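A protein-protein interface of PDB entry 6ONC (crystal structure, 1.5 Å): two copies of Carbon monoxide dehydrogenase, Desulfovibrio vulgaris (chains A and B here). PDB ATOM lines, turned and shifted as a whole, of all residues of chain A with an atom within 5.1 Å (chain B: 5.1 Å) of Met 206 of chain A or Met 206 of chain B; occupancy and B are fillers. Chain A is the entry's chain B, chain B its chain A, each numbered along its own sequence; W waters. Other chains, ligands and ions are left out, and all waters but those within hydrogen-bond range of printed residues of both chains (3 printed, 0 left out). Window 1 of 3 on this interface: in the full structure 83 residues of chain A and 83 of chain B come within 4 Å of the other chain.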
ATOM      1  N   ARG A  96     -21.405  26.346  10.295  1.00  0.00           N
ATOM      2  CA  ARG A  96     -22.282  26.567  11.442  1.00  0.00           C
ATOM      3  C   ARG A  96     -22.309  28.041  11.811  1.00  0.00           C
ATOM      4  O   ARG A  96     -23.351  28.561  12.235  1.00  0.00           O
ATOM      5  CB  ARG A  96     -21.837  25.723  12.641  1.00  0.00           C
ATOM      6  CG  ARG A  96     -22.084  24.237  12.471  1.00  0.00           C
ATOM      7  CD  ARG A  96     -22.234  23.497  13.797  1.00  0.00           C
ATOM      8  NE  ARG A  96     -22.787  22.162  13.543  1.00  0.00           N
ATOM      9  CZ  ARG A  96     -22.901  21.186  14.443  1.00  0.00           C
ATOM     10  NH1 ARG A  96     -23.423  20.018  14.072  1.00  0.00           N
ATOM     11  NH2 ARG A  96     -22.491  21.364  15.697  1.00  0.00           N
ATOM     12  N   ALA A  99     -24.683  29.549   9.467  1.00  0.00           N
ATOM     13  CA  ALA A  99     -26.039  29.127   9.796  1.00  0.00           C
ATOM     14  C   ALA A  99     -26.586  29.901  10.979  1.00  0.00           C
ATOM     15  O   ALA A  99     -27.775  30.230  11.011  1.00  0.00           O
ATOM     16  CB  ALA A  99     -26.062  27.632  10.101  1.00  0.00           C
ATOM     17  N   GLY A 100     -25.734  30.218  11.955  1.00  0.00           N
ATOM     18  CA  GLY A 100     -26.178  31.045  13.065  1.00  0.00           C
ATOM     19  C   GLY A 100     -26.662  32.413  12.618  1.00  0.00           C
ATOM     20  O   GLY A 100     -27.662  32.923  13.127  1.00  0.00           O
ATOM     21  N   ALA A 103     -29.933  32.082  10.741  1.00  0.00           N
ATOM     22  CA  ALA A 103     -31.002  31.775  11.687  1.00  0.00           C
ATOM     23  C   ALA A 103     -31.530  33.030  12.365  1.00  0.00           C
ATOM     24  O   ALA A 103     -32.734  33.132  12.624  1.00  0.00           O
ATOM     25  CB  ALA A 103     -30.511  30.772  12.734  1.00  0.00           C
ATOM     26  N   ILE A 202     -30.832  25.916   6.959  1.00  0.00           N
ATOM     27  CA  ILE A 202     -30.173  25.919   8.261  1.00  0.00           C
ATOM     28  C   ILE A 202     -30.113  24.508   8.834  1.00  0.00           C
ATOM     29  O   ILE A 202     -29.064  24.051   9.311  1.00  0.00           O
ATOM     30  CB  ILE A 202     -30.888  26.904   9.204  1.00  0.00           C
ATOM     31  CG1 ILE A 202     -30.757  28.341   8.672  1.00  0.00           C
ATOM     32  CG2 ILE A 202     -30.358  26.774  10.630  1.00  0.00           C
ATOM     33  CD1 ILE A 202     -31.770  29.311   9.310  1.00  0.00           C
ATOM     34  N   ALA A 203     -31.238  23.792   8.797  1.00  0.00           N
ATOM     35  CA  ALA A 203     -31.246  22.429   9.315  1.00  0.00           C
ATOM     36  C   ALA A 203     -30.272  21.548   8.546  1.00  0.00           C
ATOM     37  O   ALA A 203     -29.536  20.753   9.145  1.00  0.00           O
ATOM     38  CB  ALA A 203     -32.660  21.848   9.241  1.00  0.00           C
ATOM     39  N   GLU A 204     -30.262  21.664   7.216  1.00  0.00           N
ATOM     40  CA  GLU A 204     -29.336  20.852   6.435  1.00  0.00           C
ATOM     41  C   GLU A 204     -27.887  21.191   6.766  1.00  0.00           C
ATOM     42  O   GLU A 204     -27.029  20.297   6.810  1.00  0.00           O
ATOM     43  CB  GLU A 204     -29.622  20.970   4.940  1.00  0.00           C
ATOM     44  CG  GLU A 204     -28.613  20.170   4.127  1.00  0.00           C
ATOM     45  CD  GLU A 204     -28.925  20.096   2.657  1.00  0.00           C
ATOM     46  OE1 GLU A 204     -30.106  19.894   2.289  1.00  0.00           O
ATOM     47  OE2 GLU A 204     -27.968  20.212   1.863  1.00  0.00           O
ATOM     48  N   MET A 205     -27.588  22.478   7.031  1.00  0.00           N
ATOM     49  CA  MET A 205     -26.228  22.806   7.447  1.00  0.00           C
ATOM     50  C   MET A 205     -25.862  22.109   8.749  1.00  0.00           C
ATOM     51  O   MET A 205     -24.749  21.584   8.891  1.00  0.00           O
ATOM     52  CB  MET A 205     -26.021  24.312   7.587  1.00  0.00           C
ATOM     53  CG  MET A 205     -24.594  24.621   8.057  1.00  0.00           C
ATOM     54  SD  MET A 205     -23.341  24.097   6.844  1.00  0.00           S
ATOM     55  CE  MET A 205     -23.468  25.459   5.771  1.00  0.00           C
ATOM     56  N   MET A 206     -26.778  22.107   9.722  1.00  0.00           N
ATOM     57  CA  MET A 206     -26.486  21.463  10.998  1.00  0.00           C
ATOM     58  C   MET A 206     -26.327  19.956  10.842  1.00  0.00           C
ATOM     59  O   MET A 206     -25.511  19.349  11.545  1.00  0.00           O
ATOM     60  CB  MET A 206     -27.560  21.836  12.021  1.00  0.00           C
ATOM     61  CG  MET A 206     -27.562  23.342  12.348  1.00  0.00           C
ATOM     62  SD  MET A 206     -25.964  23.863  13.033  1.00  0.00           S
ATOM     63  CE  MET A 206     -25.990  22.999  14.614  1.00  0.00           C
ATOM     64  N   HIS A 207     -27.052  19.351   9.896  1.00  0.00           N
ATOM     65  CA  HIS A 207     -26.860  17.935   9.588  1.00  0.00           C
ATOM     66  C   HIS A 207     -25.499  17.691   8.940  1.00  0.00           C
ATOM     67  O   HIS A 207     -24.752  16.795   9.356  1.00  0.00           O
ATOM     68  CB  HIS A 207     -27.993  17.460   8.670  1.00  0.00           C
ATOM     69  CG  HIS A 207     -27.796  16.082   8.098  1.00  0.00           C
ATOM     70  ND1 HIS A 207     -28.347  15.702   6.894  1.00  0.00           N
ATOM     71  CD2 HIS A 207     -27.120  15.004   8.560  1.00  0.00           C
ATOM     72  CE1 HIS A 207     -28.037  14.439   6.645  1.00  0.00           C
ATOM     73  NE2 HIS A 207     -27.283  13.995   7.636  1.00  0.00           N
ATOM     74  N   ARG A 208     -25.160  18.483   7.916  1.00  0.00           N
ATOM     75  CA  ARG A 208     -23.906  18.267   7.201  1.00  0.00           C
ATOM     76  C   ARG A 208     -22.707  18.343   8.126  1.00  0.00           C
ATOM     77  O   ARG A 208     -21.712  17.640   7.914  1.00  0.00           O
ATOM     78  CB  ARG A 208     -23.747  19.291   6.080  1.00  0.00           C
ATOM     79  CG  ARG A 208     -24.621  19.036   4.866  1.00  0.00           C
ATOM     80  CD  ARG A 208     -24.384  20.141   3.828  1.00  0.00           C
ATOM     81  NE  ARG A 208     -25.237  19.966   2.656  1.00  0.00           N
ATOM     82  CZ  ARG A 208     -24.828  19.415   1.520  1.00  0.00           C
ATOM     83  NH1 ARG A 208     -25.673  19.274   0.511  1.00  0.00           N
ATOM     84  NH2 ARG A 208     -23.578  18.981   1.415  1.00  0.00           N
ATOM     85  N   THR A 209     -22.788  19.173   9.166  1.00  0.00           N
ATOM     86  CA  THR A 209     -21.658  19.415  10.047  1.00  0.00           C
ATOM     87  C   THR A 209     -21.595  18.448  11.230  1.00  0.00           C
ATOM     88  O   THR A 209     -20.625  18.496  11.993  1.00  0.00           O
ATOM     89  CB  THR A 209     -21.683  20.865  10.520  1.00  0.00           C
ATOM     90  OG1 THR A 209     -22.986  21.159  11.037  1.00  0.00           O
ATOM     91  CG2 THR A 209     -21.375  21.813   9.359  1.00  0.00           C
ATOM     92  N   HIS A 210     -22.591  17.567  11.393  1.00  0.00           N
ATOM     93  CA  HIS A 210     -22.503  16.467  12.350  1.00  0.00           C
ATOM     94  C   HIS A 210     -21.365  15.542  11.927  1.00  0.00           C
ATOM     95  O   HIS A 210     -21.042  15.438  10.740  1.00  0.00           O
ATOM     96  CB  HIS A 210     -23.829  15.689  12.333  1.00  0.00           C
ATOM     97  CG  HIS A 210     -23.951  14.625  13.388  1.00  0.00           C
ATOM     98  ND1 HIS A 210     -23.329  13.395  13.302  1.00  0.00           N
ATOM     99  CD2 HIS A 210     -24.663  14.604  14.541  1.00  0.00           C
ATOM    100  CE1 HIS A 210     -23.643  12.669  14.367  1.00  0.00           C
ATOM    101  NE2 HIS A 210     -24.439  13.389  15.141  1.00  0.00           N
ATOM    102  N   GLU A 563     -22.088  36.588  13.472  1.00  0.00           N
ATOM    103  CA  GLU A 563     -22.511  35.560  12.521  1.00  0.00           C
ATOM    104  C   GLU A 563     -23.417  36.140  11.434  1.00  0.00           C
ATOM    105  O   GLU A 563     -23.290  35.776  10.257  1.00  0.00           O
ATOM    106  CB  GLU A 563     -23.169  34.386  13.259  1.00  0.00           C
ATOM    107  CG  GLU A 563     -22.157  33.567  14.088  1.00  0.00           C
ATOM    108  CD  GLU A 563     -22.790  32.451  14.932  1.00  0.00           C
ATOM    109  OE1 GLU A 563     -23.869  32.682  15.536  1.00  0.00           O
ATOM    110  OE2 GLU A 563     -22.182  31.360  15.031  1.00  0.00           O
ATOM    111  N   ARG B  96     -26.515  24.094  20.795  1.00  0.00           N
ATOM    112  CA  ARG B  96     -26.121  23.845  19.408  1.00  0.00           C
ATOM    113  C   ARG B  96     -25.764  22.380  19.188  1.00  0.00           C
ATOM    114  O   ARG B  96     -26.029  21.820  18.112  1.00  0.00           O
ATOM    115  CB  ARG B  96     -24.964  24.760  18.990  1.00  0.00           C
ATOM    116  CG  ARG B  96     -25.399  26.194  18.778  1.00  0.00           C
ATOM    117  CD  ARG B  96     -24.429  27.011  17.945  1.00  0.00           C
ATOM    118  NE  ARG B  96     -25.050  28.295  17.641  1.00  0.00           N
ATOM    119  CZ  ARG B  96     -24.487  29.272  16.942  1.00  0.00           C
ATOM    120  NH1 ARG B  96     -25.172  30.390  16.730  1.00  0.00           N
ATOM    121  NH2 ARG B  96     -23.255  29.145  16.467  1.00  0.00           N
ATOM    122  N   ALA B  99     -28.918  20.643  18.773  1.00  0.00           N
ATOM    123  CA  ALA B  99     -29.517  21.009  17.492  1.00  0.00           C
ATOM    124  C   ALA B  99     -28.891  20.231  16.343  1.00  0.00           C
ATOM    125  O   ALA B  99     -29.581  19.867  15.382  1.00  0.00           O
ATOM    126  CB  ALA B  99     -29.387  22.516  17.248  1.00  0.00           C
ATOM    127  N   GLY B 100     -27.581  19.981  16.419  1.00  0.00           N
ATOM    128  CA  GLY B 100     -26.929  19.171  15.396  1.00  0.00           C
ATOM    129  C   GLY B 100     -27.461  17.752  15.356  1.00  0.00           C
ATOM    130  O   GLY B 100     -27.614  17.166  14.279  1.00  0.00           O
ATOM    131  N   ALA B 103     -30.923  17.893  13.894  1.00  0.00           N
ATOM    132  CA  ALA B 103     -30.859  18.150  12.460  1.00  0.00           C
ATOM    133  C   ALA B 103     -30.541  16.886  11.671  1.00  0.00           C
ATOM    134  O   ALA B 103     -31.056  16.697  10.561  1.00  0.00           O
ATOM    135  CB  ALA B 103     -29.841  19.251  12.167  1.00  0.00           C
ATOM    136  N   ILE B 202     -34.901  23.837  15.240  1.00  0.00           N
ATOM    137  CA  ILE B 202     -33.464  23.903  14.993  1.00  0.00           C
ATOM    138  C   ILE B 202     -33.048  25.321  14.638  1.00  0.00           C
ATOM    139  O   ILE B 202     -32.073  25.847  15.176  1.00  0.00           O
ATOM    140  CB  ILE B 202     -33.057  22.909  13.891  1.00  0.00           C
ATOM    141  CG1 ILE B 202     -33.299  21.478  14.364  1.00  0.00           C
ATOM    142  CG2 ILE B 202     -31.596  23.133  13.480  1.00  0.00           C
ATOM    143  CD1 ILE B 202     -33.396  20.472  13.189  1.00  0.00           C
ATOM    144  N   ALA B 203     -33.785  25.959  13.728  1.00  0.00           N
ATOM    145  CA  ALA B 203     -33.459  27.330  13.351  1.00  0.00           C
ATOM    146  C   ALA B 203     -33.552  28.257  14.555  1.00  0.00           C
ATOM    147  O   ALA B 203     -32.682  29.112  14.762  1.00  0.00           O
ATOM    148  CB  ALA B 203     -34.412  27.788  12.250  1.00  0.00           C
ATOM    149  N   GLU B 204     -34.589  28.091  15.373  1.00  0.00           N
ATOM    150  CA  GLU B 204     -34.717  28.950  16.547  1.00  0.00           C
ATOM    151  C   GLU B 204     -33.567  28.728  17.521  1.00  0.00           C
ATOM    152  O   GLU B 204     -33.117  29.667  18.189  1.00  0.00           O
ATOM    153  CB  GLU B 204     -36.068  28.749  17.243  1.00  0.00           C
ATOM    154  CG  GLU B 204     -36.173  29.653  18.470  1.00  0.00           C
ATOM    155  CD  GLU B 204     -37.521  29.656  19.159  1.00  0.00           C
ATOM    156  OE1 GLU B 204     -37.521  29.598  20.398  1.00  0.00           O
ATOM    157  OE2 GLU B 204     -38.567  29.750  18.485  1.00  0.00           O
ATOM    158  N   MET B 205     -33.082  27.490  17.631  1.00  0.00           N
ATOM    159  CA  MET B 205     -31.936  27.252  18.504  1.00  0.00           C
ATOM    160  C   MET B 205     -30.705  28.000  18.018  1.00  0.00           C
ATOM    161  O   MET B 205     -29.988  28.609  18.816  1.00  0.00           O
ATOM    162  CB  MET B 205     -31.625  25.762  18.646  1.00  0.00           C
ATOM    163  CG  MET B 205     -30.384  25.512  19.517  1.00  0.00           C
ATOM    164  SD  MET B 205     -30.580  26.066  21.237  1.00  0.00           S
ATOM    165  CE  MET B 205     -31.449  24.666  21.873  1.00  0.00           C
ATOM    166  N   MET B 206     -30.436  27.953  16.711  1.00  0.00           N
ATOM    167  CA  MET B 206     -29.299  28.675  16.162  1.00  0.00           C
ATOM    168  C   MET B 206     -29.445  30.182  16.332  1.00  0.00           C
ATOM    169  O   MET B 206     -28.442  30.880  16.521  1.00  0.00           O
ATOM    170  CB  MET B 206     -29.106  28.276  14.698  1.00  0.00           C
ATOM    171  CG  MET B 206     -28.790  26.788  14.519  1.00  0.00           C
ATOM    172  SD  MET B 206     -27.281  26.328  15.399  1.00  0.00           S
ATOM    173  CE  MET B 206     -26.042  27.265  14.488  1.00  0.00           C
ATOM    174  N   HIS B 207     -30.675  30.698  16.275  1.00  0.00           N
ATOM    175  CA  HIS B 207     -30.905  32.113  16.559  1.00  0.00           C
ATOM    176  C   HIS B 207     -30.637  32.436  18.024  1.00  0.00           C
ATOM    177  O   HIS B 207     -29.910  33.389  18.339  1.00  0.00           O
ATOM    178  CB  HIS B 207     -32.348  32.465  16.195  1.00  0.00           C
ATOM    179  CG  HIS B 207     -32.761  33.841  16.616  1.00  0.00           C
ATOM    180  ND1 HIS B 207     -34.066  34.160  16.916  1.00  0.00           N
ATOM    181  CD2 HIS B 207     -32.046  34.979  16.779  1.00  0.00           C
ATOM    182  CE1 HIS B 207     -34.141  35.442  17.236  1.00  0.00           C
ATOM    183  NE2 HIS B 207     -32.927  35.959  17.173  1.00  0.00           N
ATOM    184  N   ARG B 208     -31.226  31.653  18.935  1.00  0.00           N
ATOM    185  CA  ARG B 208     -31.061  31.907  20.366  1.00  0.00           C
ATOM    186  C   ARG B 208     -29.593  31.921  20.762  1.00  0.00           C
ATOM    187  O   ARG B 208     -29.200  32.667  21.664  1.00  0.00           O
ATOM    188  CB  ARG B 208     -31.786  30.824  21.174  1.00  0.00           C
ATOM    189  CG  ARG B 208     -33.294  31.005  21.263  1.00  0.00           C
ATOM    190  CD  ARG B 208     -33.937  29.859  22.066  1.00  0.00           C
ATOM    191  NE  ARG B 208     -35.396  29.983  22.114  1.00  0.00           N
ATOM    192  CZ  ARG B 208     -36.071  30.514  23.128  1.00  0.00           C
ATOM    193  NH1 ARG B 208     -35.423  30.983  24.185  1.00  0.00           N
ATOM    194  NH2 ARG B 208     -37.398  30.598  23.069  1.00  0.00           N
ATOM    195  N   THR B 209     -28.767  31.135  20.083  1.00  0.00           N
ATOM    196  CA  THR B 209     -27.369  30.995  20.468  1.00  0.00           C
ATOM    197  C   THR B 209     -26.436  31.985  19.767  1.00  0.00           C
ATOM    198  O   THR B 209     -25.236  31.984  20.068  1.00  0.00           O
ATOM    199  CB  THR B 209     -26.910  29.550  20.261  1.00  0.00           C
ATOM    200  OG1 THR B 209     -27.264  29.130  18.935  1.00  0.00           O
ATOM    201  CG2 THR B 209     -27.605  28.626  21.283  1.00  0.00           C
ATOM    202  N   HIS B 210     -26.948  32.813  18.850  1.00  0.00           N
ATOM    203  CA  HIS B 210     -26.200  33.962  18.335  1.00  0.00           C
ATOM    204  C   HIS B 210     -25.880  34.914  19.488  1.00  0.00           C
ATOM    205  O   HIS B 210     -26.616  34.992  20.476  1.00  0.00           O
ATOM    206  CB  HIS B 210     -27.071  34.698  17.295  1.00  0.00           C
ATOM    207  CG  HIS B 210     -26.347  35.736  16.476  1.00  0.00           C
ATOM    208  ND1 HIS B 210     -26.008  36.985  16.960  1.00  0.00           N
ATOM    209  CD2 HIS B 210     -25.942  35.716  15.181  1.00  0.00           C
ATOM    210  CE1 HIS B 210     -25.397  37.673  16.011  1.00  0.00           C
ATOM    211  NE2 HIS B 210     -25.347  36.928  14.921  1.00  0.00           N
ATOM    212  N   GLU B 563     -23.749  13.905  18.612  1.00  0.00           N
ATOM    213  CA  GLU B 563     -24.805  14.882  18.857  1.00  0.00           C
ATOM    214  C   GLU B 563     -26.181  14.225  18.795  1.00  0.00           C
ATOM    215  O   GLU B 563     -27.069  14.550  19.593  1.00  0.00           O
ATOM    216  CB  GLU B 563     -24.699  16.061  17.875  1.00  0.00           C
ATOM    217  CG  GLU B 563     -23.532  17.018  18.157  1.00  0.00           C
ATOM    218  CD  GLU B 563     -23.293  18.063  17.064  1.00  0.00           C
ATOM    219  OE1 GLU B 563     -23.469  17.752  15.865  1.00  0.00           O
ATOM    220  OE2 GLU B 563     -22.894  19.203  17.406  1.00  0.00           O
HETATM  221  O   HOH W   1     -21.253  20.954  18.851  1.00  0.00           O
HETATM  222  O   HOH W   2     -21.775  15.381  15.565  1.00  0.00           O
HETATM  223  O   HOH W   3     -23.250  35.103  17.028  1.00  0.00           O
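The side-chain carboxylate (OE2) of Glu 563 of chain B is in salt-bridge range of the guanidinium group (NH2) of Arg 96 of chain A. The side-chain sulfur (SD) of Met 206 of chain A lies close to the side-chain sulfur (SD) of Met 206 of chain B (3.7 Å). OE2 of Glu 563 of chain A lies within salt-bridge range of NH2 of Arg 96 of chain B, 2.8 Å away.
The side-chain hydroxyl (OG1) of Thr 209 of chain B sits at hydrogen-bond distance from the backbone carbonyl oxygen (O) of Met 206 of chain B. The guanidinium group of Arg 96 of chain A is in hydrogen-bond range of the side-chain hydroxyl of Thr 209 of chain A (2.7 Å). OG1 of Thr 209 of chain B is in hydrogen-bond range of NE of Arg 96 of chain B, at 2.7 Å. O of Met 206 of chain B sits at hydrogen-bond distance from NH1 of Arg 96 of chain B (3.3 Å). NH1 of Arg 96 of chain A sits at hydrogen-bond distance from O of Met 206 of chain A (3.3 Å). O of Met 206 of chain A sits at hydrogen-bond distance from OG1 of Thr 209 of chain A, 3.1 Å away.
Among the printed residues, pairs that only touch across the chains: Ala 203 of chain A with Ala 103 of chain B (3.4 Å), Ala 103 of chain A with Ala 203 of chain B (3.4 Å), Met 206 of chain A with Ala 103 of chain B (3.5 Å), Ala 103 of chain A with Met 206 of chain B (3.5 Å), Ala 103 of chain A with His 207 of chain B (3.5 Å), His 210 of chain A with Glu 563 of chain B (3.6 Å), Glu 563 of chain A with His 210 of chain B (3.6 Å), His 207 of chain A with Ala 103 of chain B (3.6 Å), Met 206 of chain A with Arg 96 of chain B (3.7 Å), Arg 96 of chain A with Met 206 of chain B (3.7 Å), Arg 96 of chain A with Gly 100 of chain B (3.8 Å), Gly 100 of chain A with Arg 96 of chain B (3.9 Å), Met 206 of chain A with Gly 100 of chain B (3.9 Å), Gly 100 of chain A with His 210 of chain B (3.9 Å), Gly 100 of chain A with Met 206 of chain B (3.9 Å) and His 210 of chain A with Gly 100 of chain B (3.9 Å).
Ile 202 of chain A touches none of the printed residues of chain B. Of chain B, only Arg 96, Gly 100, Ala 103 and Met 206 come within 4 Å of Met 206 of chain A. Printed residues of chain B within 4 Å of His 210 of chain A: Gly 100 and Glu 563. Met 206 of chain B touches just these residues of chain A: Arg 96 (3.7 Å), Gly 100 (3.9 Å), Ala 103 (3.5 Å) and Met 206 (3.7 Å). Of the printed residues of chain A, Glu 563 of chain B touches Arg 96 and His 210. The nearest residue of chain B that does not touch Met 206 of chain A is Ile 202 of chain B (4.2 Å). The nearest printed residue of chain B that does not touch His 210 of chain A is Ala 103 of chain B (6.8 Å).
Of the 14 printed residues of chain B, 8 touch a printed residue of chain A. Hydrophobic or aromatic side chains of chain A within 4 Å of the printed part of chain B: Ala 103, Met 206, His 207 and His 210. Among the printed residues, Asp or Glu carboxylates within 4 Å of a Lys or Arg side-chain nitrogen of the other chain: Arg 96 of chain A with Glu 563 of chain B (2.8 Å) and Glu 563 of chain A with Arg 96 of chain B (2.8 Å).
Arg 96 of chain A touches Met 206 of chain B, and with the chains exchanged Met 206 of chain A touches Arg 96 of chain B. Arg 96 of chain A touches Glu 563 of chain B, and with the chains exchanged Glu 563 of chain A touches Arg 96 of chain B. Ala 103 of chain A touches Ala 203 of chain B, and with the chains exchanged Ala 203 of chain A touches Ala 103 of chain B. Ala 103 of chain A touches His 207 of chain B, and with the chains exchanged His 207 of chain A touches Ala 103 of chain B. Positions printed for both chains: 96, 99, 100, 103, 202, 203, 204, 205, 206, 207, 208, 209, 210 and 563. Of the 19 pairs that touch across the chains among the printed residues, 19 have their exchanged pair printed and touching as well.
Water W1 bridges the side-chain carboxylate of Glu 563 of chain B (2.8 Å) and the guanidinium group of Arg 96 of chain A (3.4 Å). Water W3 bridges the side-chain carboxylate of Glu 563 of chain A (2.9 Å) and a ring nitrogen (ND1) of His 210 of chain B (3.3 Å). Water W2 bridges OE1 of Glu 563 of chain B and NE2 of His 210 of chain A.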
